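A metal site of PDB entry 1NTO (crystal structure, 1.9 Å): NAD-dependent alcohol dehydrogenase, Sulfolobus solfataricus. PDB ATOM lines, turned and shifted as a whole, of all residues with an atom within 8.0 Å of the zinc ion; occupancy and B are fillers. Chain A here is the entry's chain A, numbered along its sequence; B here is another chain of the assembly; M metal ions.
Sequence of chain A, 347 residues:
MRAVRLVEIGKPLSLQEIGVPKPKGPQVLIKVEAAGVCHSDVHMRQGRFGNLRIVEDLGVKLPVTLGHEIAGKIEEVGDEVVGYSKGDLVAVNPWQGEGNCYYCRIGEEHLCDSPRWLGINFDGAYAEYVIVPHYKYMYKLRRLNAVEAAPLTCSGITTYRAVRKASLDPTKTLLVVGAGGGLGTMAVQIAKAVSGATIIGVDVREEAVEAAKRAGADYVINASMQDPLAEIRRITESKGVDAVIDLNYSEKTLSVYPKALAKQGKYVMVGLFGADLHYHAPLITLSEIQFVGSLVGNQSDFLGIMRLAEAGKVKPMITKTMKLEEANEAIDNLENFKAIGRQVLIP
Residues that only touch the zinc ion: Gly 99 and Asp 113. Six residues have an atom within 4 Å of the zinc ion: Glu 98, Gly 99, Cys 101, Cys 104, Cys 112 and Asp 113. The nearest printed residue that does not touch the zinc ion is Gly 97 (4.5 Å).
The backbone NH (N) of Asn 100 is in hydrogen-bond range of the side-chain carboxylate (OE1) of Glu 98. The side-chain sulfur (SG) of Cys 101 lies close to the backbone NH (N) of Asp 113 (3.4 Å). The side-chain sulfur (SG) of Cys 101 sits close to the backbone NH (N) of Tyr 103 (3.6 Å). The side-chain sulfur (SG) of Cys 112 lies close to the backbone NH (N) of Ser 114 (3.3 Å). The side-chain sulfur of Cys 104 lies close to the backbone NH of Gly 99, 3.3 Å away. The side-chain carboxylate of Asp 113 lies within salt-bridge range of the side-chain amino group of Lys 263 of chain B (2.9 Å).
The zinc ion is bound by OE2 of Glu 98 (2.1 Å), SG of Cys 101 (2.3 Å), SG of Cys 112 (2.3 Å) and SG of Cys 104 (2.3 Å). The zinc ion has four donor atoms within binding distance.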
ATOM      1  N   GLN A  96       7.157 -14.877  25.314  1.00  0.00           N
ATOM      2  CA  GLN A  96       6.808 -15.061  26.714  1.00  0.00           C
ATOM      3  C   GLN A  96       6.076 -13.885  27.341  1.00  0.00           C
ATOM      4  O   GLN A  96       6.371 -12.727  27.054  1.00  0.00           O
ATOM      5  CB  GLN A  96       8.083 -15.382  27.476  1.00  0.00           C
ATOM      6  CG  GLN A  96       8.717 -16.701  27.011  1.00  0.00           C
ATOM      7  CD  GLN A  96      10.132 -16.914  27.529  1.00  0.00           C
ATOM      8  OE1 GLN A  96      10.530 -16.348  28.561  1.00  0.00           O
ATOM      9  NE2 GLN A  96      10.894 -17.760  26.823  1.00  0.00           N
ATOM     10  N   GLY A  97       5.119 -14.214  28.211  1.00  0.00           N
ATOM     11  CA  GLY A  97       4.326 -13.209  28.903  1.00  0.00           C
ATOM     12  C   GLY A  97       4.646 -13.136  30.393  1.00  0.00           C
ATOM     13  O   GLY A  97       5.235 -14.065  30.953  1.00  0.00           O
ATOM     14  N   GLU A  98       4.271 -12.027  31.039  1.00  0.00           N
ATOM     15  CA  GLU A  98       4.587 -11.831  32.452  1.00  0.00           C
ATOM     16  C   GLU A  98       3.583 -12.502  33.428  1.00  0.00           C
ATOM     17  O   GLU A  98       3.899 -12.696  34.600  1.00  0.00           O
ATOM     18  CB  GLU A  98       4.746 -10.330  32.743  1.00  0.00           C
ATOM     19  CG  GLU A  98       3.636  -9.431  32.175  1.00  0.00           C
ATOM     20  CD  GLU A  98       2.270  -9.737  32.797  1.00  0.00           C
ATOM     21  OE1 GLU A  98       2.186  -9.710  34.021  1.00  0.00           O
ATOM     22  OE2 GLU A  98       1.276 -10.010  32.088  1.00  0.00           O
ATOM     23  N   GLY A  99       2.398 -12.866  32.922  1.00  0.00           N
ATOM     24  CA  GLY A  99       1.468 -13.688  33.709  1.00  0.00           C
ATOM     25  C   GLY A  99       0.215 -13.026  34.262  1.00  0.00           C
ATOM     26  O   GLY A  99      -0.851 -13.644  34.360  1.00  0.00           O
ATOM     27  N   ASN A 100       0.330 -11.737  34.568  1.00  0.00           N
ATOM     28  CA  ASN A 100      -0.728 -11.006  35.235  1.00  0.00           C
ATOM     29  C   ASN A 100      -1.805 -10.392  34.337  1.00  0.00           C
ATOM     30  O   ASN A 100      -2.954 -10.289  34.744  1.00  0.00           O
ATOM     31  CB  ASN A 100      -0.104  -9.896  36.114  1.00  0.00           C
ATOM     32  CG  ASN A 100      -1.142  -9.184  36.940  1.00  0.00           C
ATOM     33  OD1 ASN A 100      -1.780  -9.784  37.823  1.00  0.00           O
ATOM     34  ND2 ASN A 100      -1.347  -7.916  36.658  1.00  0.00           N
ATOM     35  N   CYS A 101      -1.445  -9.971  33.122  1.00  0.00           N
ATOM     36  CA  CYS A 101      -2.373  -9.274  32.248  1.00  0.00           C
ATOM     37  C   CYS A 101      -3.448 -10.203  31.685  1.00  0.00           C
ATOM     38  O   CYS A 101      -3.307 -11.426  31.745  1.00  0.00           O
ATOM     39  CB  CYS A 101      -1.627  -8.592  31.090  1.00  0.00           C
ATOM     40  SG  CYS A 101      -1.143  -9.664  29.681  1.00  0.00           S
ATOM     41  N   TYR A 102      -4.508  -9.609  31.136  1.00  0.00           N
ATOM     42  CA  TYR A 102      -5.622 -10.347  30.574  1.00  0.00           C
ATOM     43  C   TYR A 102      -5.157 -11.462  29.625  1.00  0.00           C
ATOM     44  O   TYR A 102      -5.646 -12.571  29.716  1.00  0.00           O
ATOM     45  CB  TYR A 102      -6.553  -9.400  29.815  1.00  0.00           C
ATOM     46  CG  TYR A 102      -7.580 -10.076  28.934  1.00  0.00           C
ATOM     47  CD1 TYR A 102      -8.823 -10.458  29.445  1.00  0.00           C
ATOM     48  CD2 TYR A 102      -7.308 -10.352  27.593  1.00  0.00           C
ATOM     49  CE1 TYR A 102      -9.780 -11.103  28.637  1.00  0.00           C
ATOM     50  CE2 TYR A 102      -8.235 -10.983  26.790  1.00  0.00           C
ATOM     51  CZ  TYR A 102      -9.474 -11.355  27.314  1.00  0.00           C
ATOM     52  OH  TYR A 102     -10.375 -12.008  26.490  1.00  0.00           O
ATOM     53  N   TYR A 103      -4.232 -11.146  28.729  1.00  0.00           N
ATOM     54  CA  TYR A 103      -3.837 -12.108  27.687  1.00  0.00           C
ATOM     55  C   TYR A 103      -3.096 -13.285  28.276  1.00  0.00           C
ATOM     56  O   TYR A 103      -3.289 -14.427  27.854  1.00  0.00           O
ATOM     57  CB  TYR A 103      -3.027 -11.389  26.609  1.00  0.00           C
ATOM     58  CG  TYR A 103      -3.918 -10.385  25.878  1.00  0.00           C
ATOM     59  CD1 TYR A 103      -4.840 -10.808  24.922  1.00  0.00           C
ATOM     60  CD2 TYR A 103      -3.953  -9.036  26.278  1.00  0.00           C
ATOM     61  CE1 TYR A 103      -5.790  -9.926  24.380  1.00  0.00           C
ATOM     62  CE2 TYR A 103      -4.904  -8.141  25.742  1.00  0.00           C
ATOM     63  CZ  TYR A 103      -5.807  -8.593  24.800  1.00  0.00           C
ATOM     64  OH  TYR A 103      -6.735  -7.731  24.287  1.00  0.00           O
ATOM     65  N   CYS A 104      -2.252 -13.019  29.263  1.00  0.00           N
ATOM     66  CA  CYS A 104      -1.571 -14.094  29.956  1.00  0.00           C
ATOM     67  C   CYS A 104      -2.584 -14.964  30.691  1.00  0.00           C
ATOM     68  O   CYS A 104      -2.487 -16.200  30.672  1.00  0.00           O
ATOM     69  CB  CYS A 104      -0.530 -13.524  30.928  1.00  0.00           C
ATOM     70  SG  CYS A 104       0.914 -12.873  30.024  1.00  0.00           S
ATOM     71  N   ARG A 105      -3.562 -14.340  31.359  1.00  0.00           N
ATOM     72  CA  ARG A 105      -4.533 -15.127  32.097  1.00  0.00           C
ATOM     73  C   ARG A 105      -5.383 -16.045  31.212  1.00  0.00           C
ATOM     74  O   ARG A 105      -5.785 -17.127  31.650  1.00  0.00           O
ATOM     75  CB  ARG A 105      -5.452 -14.240  32.927  1.00  0.00           C
ATOM     76  CG  ARG A 105      -4.691 -13.553  34.077  1.00  0.00           C
ATOM     77  CD  ARG A 105      -5.622 -12.869  35.065  1.00  0.00           C
ATOM     78  NE  ARG A 105      -4.874 -11.956  35.924  1.00  0.00           N
ATOM     79  CZ  ARG A 105      -5.208 -11.651  37.176  1.00  0.00           C
ATOM     80  NH1 ARG A 105      -6.290 -12.197  37.734  1.00  0.00           N
ATOM     81  NH2 ARG A 105      -4.499 -10.769  37.865  1.00  0.00           N
ATOM     82  N   GLU A 108      -3.050 -16.598  26.122  1.00  0.00           N
ATOM     83  CA  GLU A 108      -2.570 -16.042  24.860  1.00  0.00           C
ATOM     84  C   GLU A 108      -1.345 -15.199  25.202  1.00  0.00           C
ATOM     85  O   GLU A 108      -1.325 -13.991  24.956  1.00  0.00           O
ATOM     86  CB  GLU A 108      -3.649 -15.155  24.227  1.00  0.00           C
ATOM     87  CG  GLU A 108      -4.954 -15.878  23.889  1.00  0.00           C
ATOM     88  CD  GLU A 108      -4.852 -16.680  22.600  1.00  0.00           C
ATOM     89  OE1 GLU A 108      -3.721 -16.952  22.157  1.00  0.00           O
ATOM     90  OE2 GLU A 108      -5.900 -17.041  22.032  1.00  0.00           O
ATOM     91  N   GLU A 109      -0.322 -15.827  25.778  1.00  0.00           N
ATOM     92  CA  GLU A 109       0.814 -15.068  26.326  1.00  0.00           C
ATOM     93  C   GLU A 109       1.584 -14.211  25.322  1.00  0.00           C
ATOM     94  O   GLU A 109       2.279 -13.259  25.730  1.00  0.00           O
ATOM     95  CB  GLU A 109       1.822 -16.014  27.027  1.00  0.00           C
ATOM     96  N   HIS A 110       1.497 -14.551  24.039  1.00  0.00           N
ATOM     97  CA  HIS A 110       2.282 -13.812  23.063  1.00  0.00           C
ATOM     98  C   HIS A 110       1.691 -12.415  22.870  1.00  0.00           C
ATOM     99  O   HIS A 110       2.377 -11.532  22.326  1.00  0.00           O
ATOM    100  CB  HIS A 110       2.300 -14.541  21.725  1.00  0.00           C
ATOM    101  CG  HIS A 110       0.937 -14.739  21.110  1.00  0.00           C
ATOM    102  ND1 HIS A 110      -0.072 -15.414  21.759  1.00  0.00           N
ATOM    103  CD2 HIS A 110       0.441 -14.365  19.907  1.00  0.00           C
ATOM    104  CE1 HIS A 110      -1.141 -15.465  20.975  1.00  0.00           C
ATOM    105  NE2 HIS A 110      -0.853 -14.840  19.840  1.00  0.00           N
ATOM    106  N   LEU A 111       0.444 -12.228  23.297  1.00  0.00           N
ATOM    107  CA  LEU A 111      -0.243 -10.921  23.193  1.00  0.00           C
ATOM    108  C   LEU A 111      -0.180 -10.141  24.502  1.00  0.00           C
ATOM    109  O   LEU A 111      -0.920  -9.175  24.708  1.00  0.00           O
ATOM    110  CB  LEU A 111      -1.710 -11.111  22.783  1.00  0.00           C
ATOM    111  CG  LEU A 111      -1.922 -11.869  21.457  1.00  0.00           C
ATOM    112  CD1 LEU A 111      -3.411 -11.991  21.178  1.00  0.00           C
ATOM    113  CD2 LEU A 111      -1.213 -11.142  20.300  1.00  0.00           C
ATOM    114  N   CYS A 112       0.702 -10.588  25.382  1.00  0.00           N
ATOM    115  CA  CYS A 112       0.984  -9.942  26.664  1.00  0.00           C
ATOM    116  C   CYS A 112       1.197  -8.429  26.571  1.00  0.00           C
ATOM    117  O   CYS A 112       1.810  -7.925  25.625  1.00  0.00           O
ATOM    118  CB  CYS A 112       2.254 -10.544  27.255  1.00  0.00           C
ATOM    119  SG  CYS A 112       2.679  -9.868  28.895  1.00  0.00           S
ATOM    120  N   ASP A 113       0.698  -7.732  27.589  1.00  0.00           N
ATOM    121  CA  ASP A 113       0.807  -6.278  27.695  1.00  0.00           C
ATOM    122  C   ASP A 113       2.216  -5.771  27.874  1.00  0.00           C
ATOM    123  O   ASP A 113       2.479  -4.613  27.602  1.00  0.00           O
ATOM    124  CB  ASP A 113       0.026  -5.751  28.902  1.00  0.00           C
ATOM    125  CG  ASP A 113      -1.438  -5.645  28.645  1.00  0.00           C
ATOM    126  OD1 ASP A 113      -1.833  -5.737  27.464  1.00  0.00           O
ATOM    127  OD2 ASP A 113      -2.165  -5.449  29.635  1.00  0.00           O
ATOM    128  N   SER A 114       3.091  -6.628  28.390  1.00  0.00           N
ATOM    129  CA  SER A 114       4.460  -6.247  28.689  1.00  0.00           C
ATOM    130  C   SER A 114       5.240  -7.482  28.356  1.00  0.00           C
ATOM    131  O   SER A 114       5.732  -8.176  29.256  1.00  0.00           O
ATOM    132  CB  SER A 114       4.579  -5.911  30.168  1.00  0.00           C
ATOM    133  OG  SER A 114       3.511  -5.049  30.552  1.00  0.00           O
ATOM    134  N   PRO A 115       5.372  -7.771  27.064  1.00  0.00           N
ATOM    135  CA  PRO A 115       6.033  -8.995  26.590  1.00  0.00           C
ATOM    136  C   PRO A 115       7.505  -9.123  26.975  1.00  0.00           C
ATOM    137  O   PRO A 115       8.205  -8.119  27.143  1.00  0.00           O
ATOM    138  CB  PRO A 115       5.809  -8.926  25.090  1.00  0.00           C
ATOM    139  CG  PRO A 115       5.811  -7.414  24.812  1.00  0.00           C
ATOM    140  CD  PRO A 115       4.999  -6.886  25.940  1.00  0.00           C
ATOM    141  N   ARG A 116       7.932 -10.380  27.160  1.00  0.00           N
ATOM    142  CA  ARG A 116       9.321 -10.698  27.412  1.00  0.00           C
ATOM    143  C   ARG A 116       9.688 -11.610  26.262  1.00  0.00           C
ATOM    144  O   ARG A 116       9.526 -12.824  26.336  1.00  0.00           O
ATOM    145  CB  ARG A 116       9.448 -11.417  28.763  1.00  0.00           C
ATOM    146  CG  ARG A 116       9.016 -10.530  29.932  1.00  0.00           C
ATOM    147  CD  ARG A 116       8.855 -11.292  31.235  1.00  0.00           C
ATOM    148  NE  ARG A 116       8.505 -10.355  32.304  1.00  0.00           N
ATOM    149  CZ  ARG A 116       8.307 -10.678  33.579  1.00  0.00           C
ATOM    150  NH1 ARG A 116       8.439 -11.938  33.991  1.00  0.00           N
ATOM    151  NH2 ARG A 116       7.993  -9.729  34.449  1.00  0.00           N
ATOM    152  N   LYS B 263      -6.367  -6.063  21.721  1.00  0.00           N
ATOM    153  CA  LYS B 263      -5.795  -7.154  20.920  1.00  0.00           C
ATOM    154  C   LYS B 263      -6.846  -8.268  20.869  1.00  0.00           C
ATOM    155  O   LYS B 263      -7.567  -8.510  21.866  1.00  0.00           O
ATOM    156  CB  LYS B 263      -4.502  -7.645  21.557  1.00  0.00           C
ATOM    157  CG  LYS B 263      -3.322  -6.689  21.344  1.00  0.00           C
ATOM    158  CD  LYS B 263      -2.145  -6.929  22.300  1.00  0.00           C
ATOM    159  CE  LYS B 263      -2.465  -6.350  23.703  1.00  0.00           C
ATOM    160  NZ  LYS B 263      -1.378  -6.528  24.750  1.00  0.00           N
HETATM  161 ZN    ZN M   1       0.876 -10.559  30.137  1.00  0.00          ZN
